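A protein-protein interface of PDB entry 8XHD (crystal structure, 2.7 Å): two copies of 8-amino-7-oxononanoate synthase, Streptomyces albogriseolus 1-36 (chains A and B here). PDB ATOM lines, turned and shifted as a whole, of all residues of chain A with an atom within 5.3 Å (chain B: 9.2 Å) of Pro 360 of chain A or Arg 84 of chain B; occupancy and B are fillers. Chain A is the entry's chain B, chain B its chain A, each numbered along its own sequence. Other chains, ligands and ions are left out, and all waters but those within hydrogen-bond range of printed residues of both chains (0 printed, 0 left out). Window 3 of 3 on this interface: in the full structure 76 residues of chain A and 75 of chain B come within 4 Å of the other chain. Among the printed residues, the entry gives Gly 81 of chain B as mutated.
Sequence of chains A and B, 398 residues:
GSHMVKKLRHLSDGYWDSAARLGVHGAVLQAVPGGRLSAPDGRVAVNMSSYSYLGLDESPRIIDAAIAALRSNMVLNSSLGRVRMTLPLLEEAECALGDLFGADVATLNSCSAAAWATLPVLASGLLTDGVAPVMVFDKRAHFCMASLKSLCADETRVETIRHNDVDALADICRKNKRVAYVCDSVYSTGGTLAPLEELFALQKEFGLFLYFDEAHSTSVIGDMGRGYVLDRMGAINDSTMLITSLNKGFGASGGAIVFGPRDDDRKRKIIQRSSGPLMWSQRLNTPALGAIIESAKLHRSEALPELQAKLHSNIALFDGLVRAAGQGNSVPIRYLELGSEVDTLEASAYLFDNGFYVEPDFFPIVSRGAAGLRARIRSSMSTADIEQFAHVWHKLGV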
ATOM      1  N   VAL A  24       0.311 -21.639  -4.648  1.00  0.00           N
ATOM      2  CA  VAL A  24       0.699 -20.272  -4.980  1.00  0.00           C
ATOM      3  C   VAL A  24       0.752 -20.032  -6.479  1.00  0.00           C
ATOM      4  O   VAL A  24       0.806 -18.874  -6.911  1.00  0.00           O
ATOM      5  CB  VAL A  24       2.061 -19.909  -4.350  1.00  0.00           C
ATOM      6  CG1 VAL A  24       1.974 -19.938  -2.830  1.00  0.00           C
ATOM      7  CG2 VAL A  24       3.146 -20.845  -4.842  1.00  0.00           C
ATOM      8  N   HIS A  25       0.730 -21.095  -7.283  1.00  0.00           N
ATOM      9  CA  HIS A  25       0.690 -20.991  -8.733  1.00  0.00           C
ATOM     10  C   HIS A  25      -0.399 -21.903  -9.280  1.00  0.00           C
ATOM     11  O   HIS A  25      -0.712 -22.945  -8.698  1.00  0.00           O
ATOM     12  CB  HIS A  25       2.036 -21.365  -9.377  1.00  0.00           C
ATOM     13  CG  HIS A  25       2.995 -20.220  -9.493  1.00  0.00           C
ATOM     14  ND1 HIS A  25       4.017 -20.198 -10.418  1.00  0.00           N
ATOM     15  CD2 HIS A  25       3.089 -19.061  -8.801  1.00  0.00           C
ATOM     16  CE1 HIS A  25       4.698 -19.073 -10.293  1.00  0.00           C
ATOM     17  NE2 HIS A  25       4.156 -18.366  -9.317  1.00  0.00           N
ATOM     18  N   GLY A  26      -0.973 -21.496 -10.411  1.00  0.00           N
ATOM     19  CA  GLY A  26      -1.911 -22.342 -11.122  1.00  0.00           C
ATOM     20  C   GLY A  26      -3.259 -22.516 -10.461  1.00  0.00           C
ATOM     21  O   GLY A  26      -3.968 -23.476 -10.771  1.00  0.00           O
ATOM     22  N   ALA A  27      -3.639 -21.611  -9.565  1.00  0.00           N
ATOM     23  CA  ALA A  27      -4.918 -21.702  -8.880  1.00  0.00           C
ATOM     24  C   ALA A  27      -5.998 -20.958  -9.657  1.00  0.00           C
ATOM     25  O   ALA A  27      -5.724 -19.989 -10.371  1.00  0.00           O
ATOM     26  CB  ALA A  27      -4.815 -21.140  -7.463  1.00  0.00           C
ATOM     27  N   THR A 344      10.886 -18.885  -0.104  1.00  0.00           N
ATOM     28  CA  THR A 344       9.990 -17.970  -0.803  1.00  0.00           C
ATOM     29  C   THR A 344       8.642 -18.627  -1.078  1.00  0.00           C
ATOM     30  O   THR A 344       7.590 -17.997  -0.918  1.00  0.00           O
ATOM     31  CB  THR A 344      10.638 -17.498  -2.106  1.00  0.00           C
ATOM     32  OG1 THR A 344      11.764 -16.664  -1.805  1.00  0.00           O
ATOM     33  CG2 THR A 344       9.650 -16.713  -2.947  1.00  0.00           C
ATOM     34  N   LEU A 345       8.655 -19.899  -1.486  1.00  0.00           N
ATOM     35  CA  LEU A 345       7.403 -20.617  -1.693  1.00  0.00           C
ATOM     36  C   LEU A 345       6.666 -20.846  -0.380  1.00  0.00           C
ATOM     37  O   LEU A 345       5.430 -20.890  -0.363  1.00  0.00           O
ATOM     38  CB  LEU A 345       7.670 -21.951  -2.389  1.00  0.00           C
ATOM     39  CG  LEU A 345       8.306 -21.892  -3.779  1.00  0.00           C
ATOM     40  CD1 LEU A 345       8.383 -23.285  -4.380  1.00  0.00           C
ATOM     41  CD2 LEU A 345       7.532 -20.955  -4.695  1.00  0.00           C
ATOM     42  N   SER A 348       5.073 -17.334   0.650  1.00  0.00           N
ATOM     43  CA  SER A 348       3.915 -17.054  -0.189  1.00  0.00           C
ATOM     44  C   SER A 348       2.739 -17.949   0.179  1.00  0.00           C
ATOM     45  O   SER A 348       1.591 -17.493   0.219  1.00  0.00           O
ATOM     46  CB  SER A 348       4.278 -17.222  -1.664  1.00  0.00           C
ATOM     47  OG  SER A 348       3.176 -16.909  -2.496  1.00  0.00           O
ATOM     48  N   TYR A 357      -2.045 -12.629  -0.839  1.00  0.00           N
ATOM     49  CA  TYR A 357      -1.280 -13.272  -1.898  1.00  0.00           C
ATOM     50  C   TYR A 357      -0.158 -12.345  -2.344  1.00  0.00           C
ATOM     51  O   TYR A 357      -0.406 -11.199  -2.736  1.00  0.00           O
ATOM     52  CB  TYR A 357      -2.171 -13.633  -3.086  1.00  0.00           C
ATOM     53  CG  TYR A 357      -1.399 -14.274  -4.223  1.00  0.00           C
ATOM     54  CD1 TYR A 357      -1.195 -15.648  -4.261  1.00  0.00           C
ATOM     55  CD2 TYR A 357      -0.859 -13.505  -5.248  1.00  0.00           C
ATOM     56  CE1 TYR A 357      -0.482 -16.238  -5.291  1.00  0.00           C
ATOM     57  CE2 TYR A 357      -0.142 -14.085  -6.280  1.00  0.00           C
ATOM     58  CZ  TYR A 357       0.042 -15.452  -6.297  1.00  0.00           C
ATOM     59  OH  TYR A 357       0.752 -16.035  -7.321  1.00  0.00           O
ATOM     60  N   VAL A 358       1.073 -12.840  -2.281  1.00  0.00           N
ATOM     61  CA  VAL A 358       2.234 -12.163  -2.845  1.00  0.00           C
ATOM     62  C   VAL A 358       2.898 -13.151  -3.791  1.00  0.00           C
ATOM     63  O   VAL A 358       3.250 -14.267  -3.382  1.00  0.00           O
ATOM     64  CB  VAL A 358       3.210 -11.686  -1.758  1.00  0.00           C
ATOM     65  CG1 VAL A 358       4.256 -10.765  -2.357  1.00  0.00           C
ATOM     66  CG2 VAL A 358       2.455 -10.988  -0.636  1.00  0.00           C
ATOM     67  N   GLU A 359       3.057 -12.756  -5.049  1.00  0.00           N
ATOM     68  CA  GLU A 359       3.535 -13.694  -6.061  1.00  0.00           C
ATOM     69  C   GLU A 359       4.996 -14.048  -5.808  1.00  0.00           C
ATOM     70  O   GLU A 359       5.809 -13.157  -5.531  1.00  0.00           O
ATOM     71  CB  GLU A 359       3.354 -13.119  -7.469  1.00  0.00           C
ATOM     72  CG  GLU A 359       4.086 -11.816  -7.740  1.00  0.00           C
ATOM     73  CD  GLU A 359       3.806 -11.276  -9.131  1.00  0.00           C
ATOM     74  OE1 GLU A 359       3.380 -12.065 -10.001  1.00  0.00           O
ATOM     75  OE2 GLU A 359       4.008 -10.062  -9.351  1.00  0.00           O
ATOM     76  N   PRO A 360       5.365 -15.328  -5.870  1.00  0.00           N
ATOM     77  CA  PRO A 360       6.751 -15.716  -5.583  1.00  0.00           C
ATOM     78  C   PRO A 360       7.638 -15.734  -6.819  1.00  0.00           C
ATOM     79  O   PRO A 360       7.319 -16.392  -7.815  1.00  0.00           O
ATOM     80  CB  PRO A 360       6.592 -17.120  -4.990  1.00  0.00           C
ATOM     81  CG  PRO A 360       5.387 -17.668  -5.692  1.00  0.00           C
ATOM     82  CD  PRO A 360       4.471 -16.495  -5.971  1.00  0.00           C
ATOM     83  N   ASP A 361       8.758 -15.020  -6.763  1.00  0.00           N
ATOM     84  CA  ASP A 361       9.733 -15.002  -7.846  1.00  0.00           C
ATOM     85  C   ASP A 361      10.857 -15.975  -7.521  1.00  0.00           C
ATOM     86  O   ASP A 361      11.562 -15.805  -6.521  1.00  0.00           O
ATOM     87  CB  ASP A 361      10.292 -13.597  -8.067  1.00  0.00           C
ATOM     88  CG  ASP A 361       9.369 -12.729  -8.892  1.00  0.00           C
ATOM     89  OD1 ASP A 361       8.218 -13.149  -9.135  1.00  0.00           O
ATOM     90  OD2 ASP A 361       9.798 -11.632  -9.306  1.00  0.00           O
ATOM     91  N   PHE A 362      11.018 -16.989  -8.363  1.00  0.00           N
ATOM     92  CA  PHE A 362      12.086 -17.966  -8.227  1.00  0.00           C
ATOM     93  C   PHE A 362      12.694 -18.225  -9.597  1.00  0.00           C
ATOM     94  O   PHE A 362      12.207 -17.738 -10.618  1.00  0.00           O
ATOM     95  CB  PHE A 362      11.577 -19.271  -7.599  1.00  0.00           C
ATOM     96  CG  PHE A 362      10.340 -19.820  -8.253  1.00  0.00           C
ATOM     97  CD1 PHE A 362      10.428 -20.580  -9.407  1.00  0.00           C
ATOM     98  CD2 PHE A 362       9.091 -19.589  -7.705  1.00  0.00           C
ATOM     99  CE1 PHE A 362       9.295 -21.090 -10.007  1.00  0.00           C
ATOM    100  CE2 PHE A 362       7.952 -20.096  -8.299  1.00  0.00           C
ATOM    101  CZ  PHE A 362       8.055 -20.848  -9.452  1.00  0.00           C
ATOM    102  N   ILE A 365      12.593 -17.212 -13.220  1.00  0.00           N
ATOM    103  CA  ILE A 365      12.128 -15.825 -13.249  1.00  0.00           C
ATOM    104  C   ILE A 365      13.196 -14.890 -12.691  1.00  0.00           C
ATOM    105  O   ILE A 365      13.369 -13.763 -13.172  1.00  0.00           O
ATOM    106  CB  ILE A 365      10.803 -15.686 -12.479  1.00  0.00           C
ATOM    107  CG1 ILE A 365       9.796 -16.743 -12.939  1.00  0.00           C
ATOM    108  CG2 ILE A 365      10.237 -14.283 -12.643  1.00  0.00           C
ATOM    109  CD1 ILE A 365       8.767 -17.095 -11.884  1.00  0.00           C
ATOM    110  N   GLY A 372      12.568 -13.791  -4.271  1.00  0.00           N
ATOM    111  CA  GLY A 372      11.905 -12.747  -3.517  1.00  0.00           C
ATOM    112  C   GLY A 372      10.406 -12.792  -3.713  1.00  0.00           C
ATOM    113  O   GLY A 372       9.881 -13.547  -4.534  1.00  0.00           O
ATOM    114  N   LEU A 373       9.717 -11.966  -2.930  1.00  0.00           N
ATOM    115  CA  LEU A 373       8.277 -11.773  -3.041  1.00  0.00           C
ATOM    116  C   LEU A 373       8.027 -10.389  -3.622  1.00  0.00           C
ATOM    117  O   LEU A 373       8.387  -9.380  -3.003  1.00  0.00           O
ATOM    118  CB  LEU A 373       7.595 -11.925  -1.683  1.00  0.00           C
ATOM    119  CG  LEU A 373       7.605 -13.327  -1.070  1.00  0.00           C
ATOM    120  CD1 LEU A 373       6.894 -13.323   0.272  1.00  0.00           C
ATOM    121  CD2 LEU A 373       6.969 -14.336  -2.014  1.00  0.00           C
ATOM    122  N   ARG A 374       7.415 -10.341  -4.802  1.00  0.00           N
ATOM    123  CA  ARG A 374       7.229  -9.095  -5.542  1.00  0.00           C
ATOM    124  C   ARG A 374       5.840  -8.547  -5.234  1.00  0.00           C
ATOM    125  O   ARG A 374       4.834  -9.042  -5.749  1.00  0.00           O
ATOM    126  CB  ARG A 374       7.432  -9.325  -7.035  1.00  0.00           C
ATOM    127  CG  ARG A 374       7.530  -8.057  -7.861  1.00  0.00           C
ATOM    128  CD  ARG A 374       8.014  -8.372  -9.269  1.00  0.00           C
ATOM    129  NE  ARG A 374       7.335  -9.532  -9.836  1.00  0.00           N
ATOM    130  CZ  ARG A 374       7.484  -9.952 -11.085  1.00  0.00           C
ATOM    131  NH1 ARG A 374       8.268  -9.316 -11.941  1.00  0.00           N
ATOM    132  NH2 ARG A 374       6.825 -11.035 -11.488  1.00  0.00           N
ATOM    133  N   SER B  78      -7.434 -10.317 -15.820  1.00  0.00           N
ATOM    134  CA  SER B  78      -6.823 -10.547 -14.521  1.00  0.00           C
ATOM    135  C   SER B  78      -5.736  -9.507 -14.272  1.00  0.00           C
ATOM    136  O   SER B  78      -5.205  -8.901 -15.206  1.00  0.00           O
ATOM    137  CB  SER B  78      -6.236 -11.958 -14.437  1.00  0.00           C
ATOM    138  OG  SER B  78      -5.183 -12.127 -15.372  1.00  0.00           O
ATOM    139  N   SER B  79      -5.415  -9.296 -12.993  1.00  0.00           N
ATOM    140  CA  SER B  79      -4.384  -8.347 -12.593  1.00  0.00           C
ATOM    141  C   SER B  79      -3.075  -9.034 -12.221  1.00  0.00           C
ATOM    142  O   SER B  79      -2.268  -8.459 -11.483  1.00  0.00           O
ATOM    143  CB  SER B  79      -4.878  -7.495 -11.427  1.00  0.00           C
ATOM    144  OG  SER B  79      -5.265  -8.310 -10.335  1.00  0.00           O
ATOM    145  N   LEU B  80      -2.853 -10.250 -12.717  1.00  0.00           N
ATOM    146  CA  LEU B  80      -1.642 -11.008 -12.445  1.00  0.00           C
ATOM    147  C   LEU B  80      -1.290 -11.826 -13.680  1.00  0.00           C
ATOM    148  O   LEU B  80      -2.127 -12.045 -14.561  1.00  0.00           O
ATOM    149  CB  LEU B  80      -1.814 -11.926 -11.225  1.00  0.00           C
ATOM    150  CG  LEU B  80      -1.580 -11.306  -9.847  1.00  0.00           C
ATOM    151  CD1 LEU B  80      -2.125 -12.205  -8.749  1.00  0.00           C
ATOM    152  CD2 LEU B  80      -0.097 -11.050  -9.635  1.00  0.00           C
ATOM    153  N   GLY B  81      -0.035 -12.266 -13.742  1.00  0.00           N
ATOM    154  CA  GLY B  81       0.384 -13.134 -14.826  1.00  0.00           C
ATOM    155  C   GLY B  81      -0.391 -14.439 -14.838  1.00  0.00           C
ATOM    156  O   GLY B  81      -0.927 -14.887 -13.824  1.00  0.00           O
ATOM    157  N   ARG B  82      -0.458 -15.051 -16.023  1.00  0.00           N
ATOM    158  CA  ARG B  82      -1.197 -16.301 -16.166  1.00  0.00           C
ATOM    159  C   ARG B  82      -0.573 -17.409 -15.330  1.00  0.00           C
ATOM    160  O   ARG B  82      -1.290 -18.211 -14.716  1.00  0.00           O
ATOM    161  CB  ARG B  82      -1.253 -16.712 -17.635  1.00  0.00           C
ATOM    162  CG  ARG B  82      -2.025 -17.995 -17.874  1.00  0.00           C
ATOM    163  CD  ARG B  82      -1.686 -18.612 -19.216  1.00  0.00           C
ATOM    164  NE  ARG B  82      -2.456 -19.828 -19.441  1.00  0.00           N
ATOM    165  CZ  ARG B  82      -3.502 -19.919 -20.251  1.00  0.00           C
ATOM    166  NH1 ARG B  82      -3.914 -18.886 -20.966  1.00  0.00           N
ATOM    167  NH2 ARG B  82      -4.145 -21.078 -20.348  1.00  0.00           N
ATOM    168  N   VAL B  83       0.763 -17.466 -15.284  1.00  0.00           N
ATOM    169  CA  VAL B  83       1.443 -18.477 -14.480  1.00  0.00           C
ATOM    170  C   VAL B  83       1.072 -18.332 -13.012  1.00  0.00           C
ATOM    171  O   VAL B  83       1.165 -19.296 -12.242  1.00  0.00           O
ATOM    172  CB  VAL B  83       2.970 -18.390 -14.679  1.00  0.00           C
ATOM    173  CG1 VAL B  83       3.359 -18.867 -16.070  1.00  0.00           C
ATOM    174  CG2 VAL B  83       3.459 -16.972 -14.442  1.00  0.00           C
ATOM    175  N   ARG B  84       0.640 -17.138 -12.602  1.00  0.00           N
ATOM    176  CA  ARG B  84       0.256 -16.915 -11.214  1.00  0.00           C
ATOM    177  C   ARG B  84      -1.143 -17.456 -10.934  1.00  0.00           C
ATOM    178  O   ARG B  84      -1.311 -18.374 -10.122  1.00  0.00           O
ATOM    179  CB  ARG B  84       0.343 -15.423 -10.883  1.00  0.00           C
ATOM    180  CG  ARG B  84       1.636 -14.753 -11.331  1.00  0.00           C
ATOM    181  CD  ARG B  84       2.860 -15.347 -10.652  1.00  0.00           C
ATOM    182  NE  ARG B  84       4.053 -14.557 -10.932  1.00  0.00           N
ATOM    183  CZ  ARG B  84       5.257 -14.811 -10.438  1.00  0.00           C
ATOM    184  NH1 ARG B  84       5.471 -15.841  -9.636  1.00  0.00           N
ATOM    185  NH2 ARG B  84       6.271 -14.012 -10.755  1.00  0.00           N
ATOM    186  N   MET B  85      -2.155 -16.909 -11.611  1.00  0.00           N
ATOM    187  CA  MET B  85      -3.540 -17.270 -11.335  1.00  0.00           C
ATOM    188  C   MET B  85      -4.386 -17.101 -12.589  1.00  0.00           C
ATOM    189  O   MET B  85      -3.989 -16.427 -13.542  1.00  0.00           O
ATOM    190  CB  MET B  85      -4.121 -16.422 -10.199  1.00  0.00           C
ATOM    191  CG  MET B  85      -3.794 -16.917  -8.805  1.00  0.00           C
ATOM    192  SD  MET B  85      -4.077 -15.626  -7.585  1.00  0.00           S
ATOM    193  CE  MET B  85      -5.095 -14.499  -8.537  1.00  0.00           C
ATOM    194  N   THR B  86      -5.571 -17.712 -12.567  1.00  0.00           N
ATOM    195  CA  THR B  86      -6.511 -17.648 -13.678  1.00  0.00           C
ATOM    196  C   THR B  86      -7.919 -17.435 -13.140  1.00  0.00           C
ATOM    197  O   THR B  86      -8.289 -17.997 -12.105  1.00  0.00           O
ATOM    198  CB  THR B  86      -6.482 -18.929 -14.527  1.00  0.00           C
ATOM    199  OG1 THR B  86      -6.738 -20.062 -13.689  1.00  0.00           O
ATOM    200  CG2 THR B  86      -5.131 -19.100 -15.211  1.00  0.00           C
ATOM    201  N   LEU B  87      -8.695 -16.613 -13.843  1.00  0.00           N
ATOM    202  CA  LEU B  87     -10.102 -16.446 -13.517  1.00  0.00           C
ATOM    203  C   LEU B  87     -10.870 -17.711 -13.909  1.00  0.00           C
ATOM    204  O   LEU B  87     -10.498 -18.393 -14.869  1.00  0.00           O
ATOM    205  CB  LEU B  87     -10.669 -15.232 -14.250  1.00  0.00           C
ATOM    206  CG  LEU B  87     -11.848 -14.460 -13.651  1.00  0.00           C
ATOM    207  CD1 LEU B  87     -11.494 -13.920 -12.274  1.00  0.00           C
ATOM    208  CD2 LEU B  87     -12.279 -13.328 -14.575  1.00  0.00           C
ATOM    209  N   GLU B  91     -10.747 -20.848 -17.456  1.00  0.00           N
ATOM    210  CA  GLU B  91     -10.702 -22.306 -17.455  1.00  0.00           C
ATOM    211  C   GLU B  91     -11.928 -22.893 -18.137  1.00  0.00           C
ATOM    212  O   GLU B  91     -11.828 -23.909 -18.835  1.00  0.00           O
ATOM    213  CB  GLU B  91     -10.576 -22.826 -16.025  1.00  0.00           C
ATOM    214  CG  GLU B  91      -9.354 -22.299 -15.288  1.00  0.00           C
ATOM    215  CD  GLU B  91      -8.047 -22.674 -15.968  1.00  0.00           C
ATOM    216  OE1 GLU B  91      -8.003 -23.718 -16.652  1.00  0.00           O
ATOM    217  OE2 GLU B  91      -7.062 -21.920 -15.824  1.00  0.00           O
ATOM    218  N   GLN B 272       4.390 -23.000 -21.506  1.00  0.00           N
ATOM    219  CA  GLN B 272       4.045 -22.052 -20.450  1.00  0.00           C
ATOM    220  C   GLN B 272       5.276 -21.656 -19.647  1.00  0.00           C
ATOM    221  O   GLN B 272       5.451 -20.481 -19.302  1.00  0.00           O
ATOM    222  CB  GLN B 272       2.976 -22.650 -19.531  1.00  0.00           C
ATOM    223  CG  GLN B 272       1.684 -21.844 -19.463  1.00  0.00           C
ATOM    224  CD  GLN B 272       0.527 -22.643 -18.882  1.00  0.00           C
ATOM    225  OE1 GLN B 272       0.727 -23.657 -18.212  1.00  0.00           O
ATOM    226  NE2 GLN B 272      -0.694 -22.190 -19.145  1.00  0.00           N
ATOM    227  N   LEU B 278       2.981 -16.750 -23.965  1.00  0.00           N
ATOM    228  CA  LEU B 278       2.129 -17.511 -23.057  1.00  0.00           C
ATOM    229  C   LEU B 278       2.485 -17.271 -21.593  1.00  0.00           C
ATOM    230  O   LEU B 278       1.652 -17.519 -20.715  1.00  0.00           O
ATOM    231  CB  LEU B 278       2.214 -19.004 -23.381  1.00  0.00           C
ATOM    232  CG  LEU B 278       1.155 -19.897 -22.728  1.00  0.00           C
ATOM    233  CD1 LEU B 278      -0.229 -19.358 -23.031  1.00  0.00           C
ATOM    234  CD2 LEU B 278       1.275 -21.341 -23.188  1.00  0.00           C
ATOM    235  N   MET B 279       3.694 -16.782 -21.315  1.00  0.00           N
ATOM    236  CA  MET B 279       4.145 -16.505 -19.956  1.00  0.00           C
ATOM    237  C   MET B 279       4.083 -15.029 -19.591  1.00  0.00           C
ATOM    238  O   MET B 279       3.690 -14.697 -18.467  1.00  0.00           O
ATOM    239  CB  MET B 279       5.586 -17.001 -19.761  1.00  0.00           C
ATOM    240  CG  MET B 279       6.231 -16.558 -18.454  1.00  0.00           C
ATOM    241  SD  MET B 279       8.005 -16.901 -18.342  1.00  0.00           S
ATOM    242  CE  MET B 279       8.004 -18.672 -18.075  1.00  0.00           C
ATOM    243  N   ARG B 283      -3.689 -12.000 -20.997  1.00  0.00           N
ATOM    244  CA  ARG B 283      -4.703 -12.970 -21.377  1.00  0.00           C
ATOM    245  C   ARG B 283      -5.873 -12.272 -22.059  1.00  0.00           C
ATOM    246  O   ARG B 283      -6.046 -11.055 -21.955  1.00  0.00           O
ATOM    247  CB  ARG B 283      -5.205 -13.737 -20.156  1.00  0.00           C
ATOM    248  CG  ARG B 283      -4.126 -14.465 -19.377  1.00  0.00           C
ATOM    249  CD  ARG B 283      -3.768 -15.802 -20.009  1.00  0.00           C
ATOM    250  NE  ARG B 283      -2.815 -15.686 -21.107  1.00  0.00           N
ATOM    251  CZ  ARG B 283      -3.123 -15.831 -22.388  1.00  0.00           C
ATOM    252  NH1 ARG B 283      -4.357 -16.111 -22.774  1.00  0.00           N
ATOM    253  NH2 ARG B 283      -2.169 -15.693 -23.304  1.00  0.00           N
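NE2 of His 25 of chain A lies within hydrogen-bond range of NH1 of Arg 84 of chain B (2.9 Å).
The backbone NH of Thr 86 of chain B is in hydrogen-bond range of the backbone carbonyl oxygen of Ala 27 of chain A.
NH2 of Arg 84 of chain B is in salt-bridge range of OD1 of Asp 361 of chain A.
NH2 of Arg 374 of chain A sits close to NH2 of Arg 84 of chain B (3.1 Å).
N of Gly 26 of chain A sits at hydrogen-bond distance from O of Arg 84 of chain B, 3.2 Å away.
The backbone carbonyl oxygen of Pro 360 of chain A lies within hydrogen-bond range of the guanidinium group of Arg 84 of chain B (2.7 Å).
NE of Arg 84 of chain B lies within salt-bridge range of OE1 of Glu 359 of chain A.
No position is printed for both chains.
Of the 14 pairs that touch across the chains among the printed residues, none has its exchanged pair printed and touching as well.
Printed residues of chain A that touch a printed residue of chain B: Val 24, His 25, Gly 26, Ala 27, Tyr 357, Glu 359, Pro 360, Asp 361 and Arg 374.
Hydrophobic or aromatic side chains of chain A within 4 Å of the printed part of chain B: His 25, Tyr 357 and Pro 360.
Hydrophobic or aromatic side chains of chain B within 4 Å of the printed part of chain A: Leu 80 and Met 85.
Among the printed residues, Asp or Glu carboxylates within 4 Å of a Lys or Arg side-chain nitrogen of the other chain: Glu 359 of chain A with Arg 84 of chain B (2.7 Å) and Asp 361 of chain A with Arg 84 of chain B (2.7 Å).
The backbone NH (N) of Asp 361 of chain A is in hydrogen-bond range of the backbone carbonyl oxygen (O) of Gly 372 of chain A, at 2.9 Å.
The side-chain hydroxyl (OG1) of Thr 86 of chain B lies within hydrogen-bond range of the side-chain carboxylate (OE2) of Glu 91 of chain B (2.8 Å).
The side-chain carboxylate (OD2) of Asp 361 of chain A is in salt-bridge range of the guanidinium group (NE) of Arg 374 of chain A (3.3 Å).
The backbone carbonyl oxygen of Leu 80 of chain B is in hydrogen-bond range of the side-chain hydroxyl of Ser 78 of chain B.
OE2 of Glu 359 of chain A lies within salt-bridge range of NE of Arg 374 of chain A, at 3.4 Å.
OH of Tyr 357 of chain A is in hydrogen-bond range of O of Val 24 of chain A (2.9 Å).
Among the printed residues, pairs that only touch across the chains: Val 24 of chain A with Arg 84 of chain B (3.9 Å), His 25 of chain A with Val 83 of chain B (3.4 Å), Gly 26 of chain A with Val 83 of chain B (3.6 Å), Ala 27 of chain A with Met 85 of chain B (3.6 Å), Tyr 357 of chain A with Leu 80 of chain B (3.7 Å), Tyr 357 of chain A with Arg 84 of chain B (3.6 Å) and Glu 359 of chain A with Leu 80 of chain B (3.6 Å).
Printed residues of chain B within 4 Å of Gly 26 of chain A: Val 83 (3.6 Å) and Arg 84 (3.2 Å).
Printed residues of chain B within 4 Å of Ala 27 of chain A: Met 85 (3.6 Å) and Thr 86 (3.2 Å).
Thr 344 of chain A touches none of the printed residues of chain B.
Glu 359 of chain A touches just these residues of chain B: Leu 80 and Arg 84.
Pro 360 of chain A touches one residue of chain B.
Asp 361 of chain A touches one residue of chain B.
Printed residues of chain A within 4 Å of Val 83 of chain B: His 25 (3.4 Å) and Gly 26 (3.6 Å).
Of the printed residues of chain A, Arg 84 of chain B touches Val 24 (3.9 Å), His 25 (2.9 Å), Gly 26 (3.2 Å), Tyr 357 (3.6 Å), Glu 359 (2.7 Å), Pro 360 (2.7 Å), Asp 361 (2.7 Å) and Arg 374 (3.1 Å).
Of the printed residues of chain A, Met 85 of chain B touches Ala 27 (3.6 Å).
Met 279 of chain B touches none of the printed residues of chain A.
The nearest residue of chain B that does not touch Pro 360 of chain A is Val 83 of chain B (7.6 Å).
The nearest residue of chain A that does not touch Arg 84 of chain B is Ala 27 of chain A (4.03 Å).
The nearest printed residue of chain B that does not touch Arg 374 of chain A is Leu 80 of chain B (6.6 Å).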
